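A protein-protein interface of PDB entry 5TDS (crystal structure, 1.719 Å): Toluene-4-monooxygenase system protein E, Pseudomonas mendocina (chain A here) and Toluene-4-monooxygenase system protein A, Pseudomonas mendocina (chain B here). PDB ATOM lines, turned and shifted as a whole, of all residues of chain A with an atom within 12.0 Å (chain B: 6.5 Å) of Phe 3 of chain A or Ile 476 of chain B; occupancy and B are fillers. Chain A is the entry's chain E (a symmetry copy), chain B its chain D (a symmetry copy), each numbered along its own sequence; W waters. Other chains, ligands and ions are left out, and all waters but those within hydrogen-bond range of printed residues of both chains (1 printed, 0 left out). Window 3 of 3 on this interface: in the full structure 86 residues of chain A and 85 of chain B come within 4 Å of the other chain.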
ATOM      1  N   PHE A   3      11.786 -18.549 -29.570  1.00  0.00           N
ATOM      2  CA  PHE A   3      12.990 -18.300 -28.776  1.00  0.00           C
ATOM      3  C   PHE A   3      13.181 -16.820 -28.492  1.00  0.00           C
ATOM      4  O   PHE A   3      12.940 -15.977 -29.350  1.00  0.00           O
ATOM      5  CB  PHE A   3      14.233 -18.842 -29.484  1.00  0.00           C
ATOM      6  CG  PHE A   3      14.301 -20.338 -29.524  1.00  0.00           C
ATOM      7  CD1 PHE A   3      14.713 -21.054 -28.411  1.00  0.00           C
ATOM      8  CD2 PHE A   3      13.953 -21.029 -30.674  1.00  0.00           C
ATOM      9  CE1 PHE A   3      14.773 -22.436 -28.442  1.00  0.00           C
ATOM     10  CE2 PHE A   3      14.014 -22.406 -30.716  1.00  0.00           C
ATOM     11  CZ  PHE A   3      14.429 -23.113 -29.597  1.00  0.00           C
ATOM     12  N   GLU A   4      13.622 -16.497 -27.286  1.00  0.00           N
ATOM     13  CA  GLU A   4      13.878 -15.107 -26.966  1.00  0.00           C
ATOM     14  C   GLU A   4      15.364 -14.851 -26.778  1.00  0.00           C
ATOM     15  O   GLU A   4      16.177 -15.777 -26.773  1.00  0.00           O
ATOM     16  CB  GLU A   4      13.103 -14.689 -25.718  1.00  0.00           C
ATOM     17  CG  GLU A   4      13.204 -15.655 -24.564  1.00  0.00           C
ATOM     18  CD  GLU A   4      12.351 -15.231 -23.390  1.00  0.00           C
ATOM     19  OE1 GLU A   4      11.653 -16.093 -22.816  1.00  0.00           O
ATOM     20  OE2 GLU A   4      12.380 -14.030 -23.040  1.00  0.00           O
ATOM     21  N   SER A   5      15.710 -13.580 -26.641  1.00  0.00           N
ATOM     22  CA  SER A   5      17.083 -13.182 -26.391  1.00  0.00           C
ATOM     23  C   SER A   5      17.371 -13.215 -24.895  1.00  0.00           C
ATOM     24  O   SER A   5      16.592 -12.696 -24.097  1.00  0.00           O
ATOM     25  CB  SER A   5      17.343 -11.783 -26.955  1.00  0.00           C
ATOM     26  OG  SER A   5      18.646 -11.341 -26.613  1.00  0.00           O
ATOM     27  N   LYS A   6      18.483 -13.839 -24.517  1.00  0.00           N
ATOM     28  CA  LYS A   6      18.878 -13.887 -23.116  1.00  0.00           C
ATOM     29  C   LYS A   6      20.343 -13.502 -22.952  1.00  0.00           C
ATOM     30  O   LYS A   6      21.156 -13.756 -23.839  1.00  0.00           O
ATOM     31  CB  LYS A   6      18.628 -15.281 -22.545  1.00  0.00           C
ATOM     32  CG  LYS A   6      17.162 -15.683 -22.516  1.00  0.00           C
ATOM     33  CD  LYS A   6      17.001 -17.071 -21.947  1.00  0.00           C
ATOM     34  CE  LYS A   6      15.552 -17.515 -21.972  1.00  0.00           C
ATOM     35  NZ  LYS A   6      15.440 -18.926 -21.510  1.00  0.00           N
ATOM     36  N   LYS A   7      20.669 -12.888 -21.816  1.00  0.00           N
ATOM     37  CA  LYS A   7      22.042 -12.519 -21.487  1.00  0.00           C
ATOM     38  C   LYS A   7      22.893 -13.746 -21.190  1.00  0.00           C
ATOM     39  O   LYS A   7      22.365 -14.797 -20.831  1.00  0.00           O
ATOM     40  CB  LYS A   7      22.082 -11.603 -20.260  1.00  0.00           C
ATOM     41  CG  LYS A   7      21.328 -10.293 -20.360  1.00  0.00           C
ATOM     42  CD  LYS A   7      21.380  -9.595 -18.998  1.00  0.00           C
ATOM     43  CE  LYS A   7      20.749  -8.214 -19.022  1.00  0.00           C
ATOM     44  NZ  LYS A   7      21.581  -7.206 -19.756  1.00  0.00           N
ATOM     45  N   PRO A   8      24.224 -13.610 -21.305  1.00  0.00           N
ATOM     46  CA  PRO A   8      25.064 -14.713 -20.847  1.00  0.00           C
ATOM     47  C   PRO A   8      24.873 -14.958 -19.362  1.00  0.00           C
ATOM     48  O   PRO A   8      24.495 -14.044 -18.621  1.00  0.00           O
ATOM     49  CB  PRO A   8      26.491 -14.229 -21.145  1.00  0.00           C
ATOM     50  CG  PRO A   8      26.322 -13.198 -22.214  1.00  0.00           C
ATOM     51  CD  PRO A   8      25.019 -12.520 -21.890  1.00  0.00           C
ATOM     52  N   MET A   9      25.124 -16.195 -18.947  1.00  0.00           N
ATOM     53  CA  MET A   9      25.094 -16.577 -17.546  1.00  0.00           C
ATOM     54  C   MET A   9      26.523 -16.611 -17.030  1.00  0.00           C
ATOM     55  O   MET A   9      27.432 -17.013 -17.745  1.00  0.00           O
ATOM     56  CB  MET A   9      24.411 -17.937 -17.375  1.00  0.00           C
ATOM     57  CG  MET A   9      22.960 -17.939 -17.836  1.00  0.00           C
ATOM     58  SD  MET A   9      22.286 -19.578 -18.180  1.00  0.00           S
ATOM     59  CE  MET A   9      23.200 -20.032 -19.658  1.00  0.00           C
ATOM     60  N   LEU B 464      10.881 -28.052 -37.210  1.00  0.00           N
ATOM     61  CA  LEU B 464      12.286 -27.941 -36.829  1.00  0.00           C
ATOM     62  C   LEU B 464      12.400 -27.081 -35.573  1.00  0.00           C
ATOM     63  O   LEU B 464      13.219 -27.361 -34.698  1.00  0.00           O
ATOM     64  CB  LEU B 464      13.129 -27.361 -37.968  1.00  0.00           C
ATOM     65  CG  LEU B 464      14.654 -27.401 -37.814  1.00  0.00           C
ATOM     66  CD1 LEU B 464      15.153 -28.820 -37.530  1.00  0.00           C
ATOM     67  CD2 LEU B 464      15.321 -26.845 -39.062  1.00  0.00           C
ATOM     68  N   GLU B 465      11.563 -26.050 -35.467  1.00  0.00           N
ATOM     69  CA  GLU B 465      11.566 -25.214 -34.269  1.00  0.00           C
ATOM     70  C   GLU B 465      11.200 -25.995 -33.005  1.00  0.00           C
ATOM     71  O   GLU B 465      11.801 -25.795 -31.944  1.00  0.00           O
ATOM     72  CB  GLU B 465      10.609 -24.041 -34.421  1.00  0.00           C
ATOM     73  CG  GLU B 465      10.464 -23.247 -33.140  1.00  0.00           C
ATOM     74  CD  GLU B 465       9.995 -21.836 -33.391  1.00  0.00           C
ATOM     75  OE1 GLU B 465       8.820 -21.661 -33.778  1.00  0.00           O
ATOM     76  OE2 GLU B 465      10.808 -20.903 -33.210  1.00  0.00           O
ATOM     77  N   GLY B 466      10.202 -26.867 -33.115  1.00  0.00           N
ATOM     78  CA  GLY B 466       9.861 -27.760 -32.025  1.00  0.00           C
ATOM     79  C   GLY B 466      11.047 -28.640 -31.677  1.00  0.00           C
ATOM     80  O   GLY B 466      11.311 -28.918 -30.500  1.00  0.00           O
ATOM     81  N   ALA B 467      11.757 -29.086 -32.709  1.00  0.00           N
ATOM     82  CA  ALA B 467      12.953 -29.906 -32.520  1.00  0.00           C
ATOM     83  C   ALA B 467      14.048 -29.135 -31.790  1.00  0.00           C
ATOM     84  O   ALA B 467      14.751 -29.698 -30.953  1.00  0.00           O
ATOM     85  CB  ALA B 467      13.475 -30.411 -33.860  1.00  0.00           C
ATOM     86  N   LEU B 468      14.205 -27.852 -32.117  1.00  0.00           N
ATOM     87  CA  LEU B 468      15.227 -27.041 -31.466  1.00  0.00           C
ATOM     88  C   LEU B 468      14.933 -26.928 -29.970  1.00  0.00           C
ATOM     89  O   LEU B 468      15.844 -26.974 -29.148  1.00  0.00           O
ATOM     90  CB  LEU B 468      15.318 -25.656 -32.110  1.00  0.00           C
ATOM     91  CG  LEU B 468      15.880 -25.630 -33.534  1.00  0.00           C
ATOM     92  CD1 LEU B 468      15.624 -24.275 -34.193  1.00  0.00           C
ATOM     93  CD2 LEU B 468      17.384 -25.962 -33.543  1.00  0.00           C
ATOM     94  N   LYS B 469      13.661 -26.788 -29.608  1.00  0.00           N
ATOM     95  CA  LYS B 469      13.285 -26.730 -28.201  1.00  0.00           C
ATOM     96  C   LYS B 469      13.615 -28.047 -27.504  1.00  0.00           C
ATOM     97  O   LYS B 469      14.146 -28.070 -26.383  1.00  0.00           O
ATOM     98  CB  LYS B 469      11.793 -26.416 -28.062  1.00  0.00           C
ATOM     99  CG  LYS B 469      11.404 -25.014 -28.504  1.00  0.00           C
ATOM    100  CD  LYS B 469      11.762 -23.988 -27.437  1.00  0.00           C
ATOM    101  CE  LYS B 469      11.103 -22.642 -27.708  1.00  0.00           C
ATOM    102  NZ  LYS B 469      11.339 -21.712 -26.573  1.00  0.00           N
ATOM    103  N   TYR B 470      13.294 -29.146 -28.177  1.00  0.00           N
ATOM    104  CA  TYR B 470      13.548 -30.479 -27.653  1.00  0.00           C
ATOM    105  C   TYR B 470      15.042 -30.686 -27.455  1.00  0.00           C
ATOM    106  O   TYR B 470      15.473 -31.348 -26.511  1.00  0.00           O
ATOM    107  CB  TYR B 470      12.982 -31.535 -28.603  1.00  0.00           C
ATOM    108  CG  TYR B 470      13.301 -32.949 -28.201  1.00  0.00           C
ATOM    109  CD1 TYR B 470      12.556 -33.594 -27.221  1.00  0.00           C
ATOM    110  CD2 TYR B 470      14.336 -33.652 -28.810  1.00  0.00           C
ATOM    111  CE1 TYR B 470      12.842 -34.889 -26.848  1.00  0.00           C
ATOM    112  CE2 TYR B 470      14.630 -34.959 -28.438  1.00  0.00           C
ATOM    113  CZ  TYR B 470      13.876 -35.566 -27.458  1.00  0.00           C
ATOM    114  OH  TYR B 470      14.150 -36.856 -27.079  1.00  0.00           O
ATOM    115  N   GLY B 472      17.148 -28.628 -26.521  1.00  0.00           N
ATOM    116  CA  GLY B 472      17.632 -27.969 -25.323  1.00  0.00           C
ATOM    117  C   GLY B 472      18.130 -26.547 -25.488  1.00  0.00           C
ATOM    118  O   GLY B 472      18.711 -25.994 -24.562  1.00  0.00           O
ATOM    119  N   PHE B 473      17.902 -25.935 -26.646  1.00  0.00           N
ATOM    120  CA  PHE B 473      18.298 -24.537 -26.807  1.00  0.00           C
ATOM    121  C   PHE B 473      17.411 -23.646 -25.940  1.00  0.00           C
ATOM    122  O   PHE B 473      16.201 -23.879 -25.808  1.00  0.00           O
ATOM    123  CB  PHE B 473      18.260 -24.126 -28.288  1.00  0.00           C
ATOM    124  CG  PHE B 473      19.353 -24.767 -29.101  1.00  0.00           C
ATOM    125  CD1 PHE B 473      20.638 -24.242 -29.092  1.00  0.00           C
ATOM    126  CD2 PHE B 473      19.113 -25.940 -29.812  1.00  0.00           C
ATOM    127  CE1 PHE B 473      21.654 -24.859 -29.809  1.00  0.00           C
ATOM    128  CE2 PHE B 473      20.131 -26.565 -30.525  1.00  0.00           C
ATOM    129  CZ  PHE B 473      21.400 -26.023 -30.528  1.00  0.00           C
ATOM    130  N   GLN B 474      18.026 -22.640 -25.328  1.00  0.00           N
ATOM    131  CA  GLN B 474      17.323 -21.802 -24.349  1.00  0.00           C
ATOM    132  C   GLN B 474      17.237 -20.330 -24.743  1.00  0.00           C
ATOM    133  O   GLN B 474      16.530 -19.552 -24.097  1.00  0.00           O
ATOM    134  CB  GLN B 474      17.992 -21.931 -22.979  1.00  0.00           C
ATOM    135  CG  GLN B 474      17.806 -23.298 -22.343  1.00  0.00           C
ATOM    136  CD  GLN B 474      18.579 -23.467 -21.041  1.00  0.00           C
ATOM    137  OE1 GLN B 474      19.076 -22.494 -20.466  1.00  0.00           O
ATOM    138  NE2 GLN B 474      18.688 -24.712 -20.572  1.00  0.00           N
ATOM    139  N   SER B 475      17.949 -19.937 -25.792  1.00  0.00           N
ATOM    140  CA  SER B 475      17.844 -18.566 -26.282  1.00  0.00           C
ATOM    141  C   SER B 475      18.276 -18.491 -27.739  1.00  0.00           C
ATOM    142  O   SER B 475      18.891 -19.422 -28.259  1.00  0.00           O
ATOM    143  CB  SER B 475      18.676 -17.608 -25.415  1.00  0.00           C
ATOM    144  OG  SER B 475      20.055 -17.651 -25.754  1.00  0.00           O
ATOM    145  N   ILE B 476      17.929 -17.389 -28.401  1.00  0.00           N
ATOM    146  CA  ILE B 476      18.331 -17.166 -29.784  1.00  0.00           C
ATOM    147  C   ILE B 476      19.840 -17.230 -29.956  1.00  0.00           C
ATOM    148  O   ILE B 476      20.343 -17.763 -30.946  1.00  0.00           O
ATOM    149  CB  ILE B 476      17.855 -15.794 -30.302  1.00  0.00           C
ATOM    150  CG1 ILE B 476      16.350 -15.804 -30.528  1.00  0.00           C
ATOM    151  CG2 ILE B 476      18.569 -15.436 -31.604  1.00  0.00           C
ATOM    152  CD1 ILE B 476      15.855 -14.560 -31.222  1.00  0.00           C
ATOM    153  N   GLU B 477      20.557 -16.663 -28.989  1.00  0.00           N
ATOM    154  CA  GLU B 477      22.012 -16.572 -29.056  1.00  0.00           C
ATOM    155  C   GLU B 477      22.718 -17.925 -29.072  1.00  0.00           C
ATOM    156  O   GLU B 477      23.840 -18.029 -29.559  1.00  0.00           O
ATOM    157  CB  GLU B 477      22.543 -15.745 -27.877  1.00  0.00           C
ATOM    158  CG  GLU B 477      22.167 -14.270 -27.936  1.00  0.00           C
ATOM    159  CD  GLU B 477      20.814 -13.971 -27.319  1.00  0.00           C
ATOM    160  OE1 GLU B 477      20.165 -14.901 -26.794  1.00  0.00           O
ATOM    161  OE2 GLU B 477      20.399 -12.790 -27.360  1.00  0.00           O
ATOM    162  N   GLU B 478      22.074 -18.958 -28.535  1.00  0.00           N
ATOM    163  CA  GLU B 478      22.724 -20.255 -28.393  1.00  0.00           C
ATOM    164  C   GLU B 478      22.773 -21.024 -29.702  1.00  0.00           C
ATOM    165  O   GLU B 478      23.627 -21.896 -29.902  1.00  0.00           O
ATOM    166  CB  GLU B 478      22.011 -21.098 -27.335  1.00  0.00           C
ATOM    167  CG  GLU B 478      22.096 -20.501 -25.943  1.00  0.00           C
ATOM    168  CD  GLU B 478      21.398 -21.347 -24.906  1.00  0.00           C
ATOM    169  OE1 GLU B 478      20.892 -22.434 -25.260  1.00  0.00           O
ATOM    170  OE2 GLU B 478      21.355 -20.924 -23.733  1.00  0.00           O
ATOM    171  N   MET B 479      21.854 -20.712 -30.599  1.00  0.00           N
ATOM    172  CA  MET B 479      21.788 -21.457 -31.839  1.00  0.00           C
ATOM    173  C   MET B 479      22.881 -21.043 -32.815  1.00  0.00           C
ATOM    174  O   MET B 479      23.242 -19.863 -32.914  1.00  0.00           O
ATOM    175  CB  MET B 479      20.408 -21.299 -32.452  1.00  0.00           C
ATOM    176  CG  MET B 479      19.376 -21.965 -31.587  1.00  0.00           C
ATOM    177  SD  MET B 479      17.776 -21.971 -32.359  1.00  0.00           S
ATOM    178  CE  MET B 479      17.406 -20.234 -32.307  1.00  0.00           C
ATOM    179  N   GLY B 480      23.411 -22.035 -33.522  1.00  0.00           N
ATOM    180  CA  GLY B 480      24.506 -21.819 -34.459  1.00  0.00           C
ATOM    181  C   GLY B 480      24.163 -20.841 -35.566  1.00  0.00           C
ATOM    182  O   GLY B 480      23.068 -20.859 -36.122  1.00  0.00           O
ATOM    183  N   LYS B 481      25.122 -19.983 -35.879  1.00  0.00           N
ATOM    184  CA  LYS B 481      25.024 -19.053 -36.999  1.00  0.00           C
ATOM    185  C   LYS B 481      26.270 -19.192 -37.845  1.00  0.00           C
ATOM    186  O   LYS B 481      27.240 -19.837 -37.423  1.00  0.00           O
ATOM    187  CB  LYS B 481      24.906 -17.611 -36.515  1.00  0.00           C
ATOM    188  CG  LYS B 481      23.755 -17.314 -35.578  1.00  0.00           C
ATOM    189  CD  LYS B 481      24.057 -16.020 -34.814  1.00  0.00           C
ATOM    190  CE  LYS B 481      22.806 -15.373 -34.240  1.00  0.00           C
ATOM    191  NZ  LYS B 481      22.142 -14.495 -35.249  1.00  0.00           N
HETATM  192  O   HOH W   1      13.884 -18.725 -25.391  1.00  0.00           O
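Of the 17 printed residues of chain B, 8 touch a printed residue of chain A.
Printed residues of chain B that touch a printed residue of chain A: Leu 468, Lys 469, Phe 473, Gln 474, Ser 475, Ile 476, Glu 477 and Met 479.
Hydrophobic or aromatic side chains of chain B within 4 Å of the printed part of chain A: Leu 468, Phe 473, Ile 476 and Met 479.
Hydrophobic or aromatic side chains of chain A that line the printed part of chain B: Phe 3.
Among the printed residues, 11 pairs touch across the chains.
Among the printed residues, no Asp or Glu carboxylate lies within 4 Å of a Lys or Arg side-chain nitrogen of the other chain.
Water W1 lies within hydrogen-bond range of N of Glu 4 of chain A (2.9 Å) and O of Gln 474 of chain B (3.1 Å).
The backbone carbonyl oxygen of Leu 468 of chain B is in hydrogen-bond range of the backbone NH of Phe 473 of chain B (3.4 Å).
OE1 of Glu 478 of chain B is in hydrogen-bond range of N of Gln 474 of chain B (2.9 Å).
The side-chain hydroxyl (OG) of Ser 475 of chain B lies within hydrogen-bond range of the side-chain carboxylate (OE1) of Glu 477 of chain B, at 2.9 Å.
Among the printed residues, merely in contact across the chains: Glu 4 of chain A with Ser 475 of chain B (3.3 Å), Phe 3 of chain A with Phe 473 of chain B (3.3 Å), Phe 3 of chain A with Lys 469 of chain B (3.5 Å), Phe 3 of chain A with Ile 476 of chain B (3.6 Å), Phe 3 of chain A with Leu 468 of chain B (3.7 Å), Lys 6 of chain A with Ser 475 of chain B (3.7 Å) and Phe 3 of chain A with Met 479 of chain B (3.9 Å).
NZ of Lys 6 of chain A is in hydrogen-bond range of O of Gln 474 of chain B.
N of Ile 476 of chain B lies within hydrogen-bond range of O of Glu 4 of chain A, 2.9 Å away.
The backbone NH of Lys 6 of chain A lies within hydrogen-bond range of the side-chain carboxylate of Glu 477 of chain B.
The side-chain carboxylate (OE2) of Glu 477 of chain B lies close to the side-chain hydroxyl (OG) of Ser 5 of chain A (2.4 Å).
Printed residues of chain A within 4 Å of Ile 476 of chain B: Phe 3 and Glu 4.
No residue of chain A comes within 4 Å of Glu 465 of chain B.
No residue of chain A comes within 4 Å of Gly 466 of chain B.
Of chain A, only Phe 3 comes within 4 Å of Leu 468 of chain B.
No residue of chain A comes within 4 Å of Gly 472 of chain B.
Ser 475 of chain B touches two residues of chain A.
Glu 477 of chain B touches two residues of chain A.
No residue of chain A comes within 4 Å of Glu 478 of chain B.
Of the printed residues of chain A, Met 479 of chain B touches Phe 3 (3.9 Å).
No residue of chain A comes within 4 Å of Gly 480 of chain B.
Of the printed residues of chain B, Ser 5 of chain A touches Glu 477.
Of the printed residues of chain A, Gln 474 of chain B touches Lys 6.
Printed residues of chain A within 4 Å of Lys 469 of chain B: Phe 3 (3.5 Å).
The nearest printed residue of chain B that does not touch Ser 5 of chain A is Ile 476 of chain B (4.5 Å).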
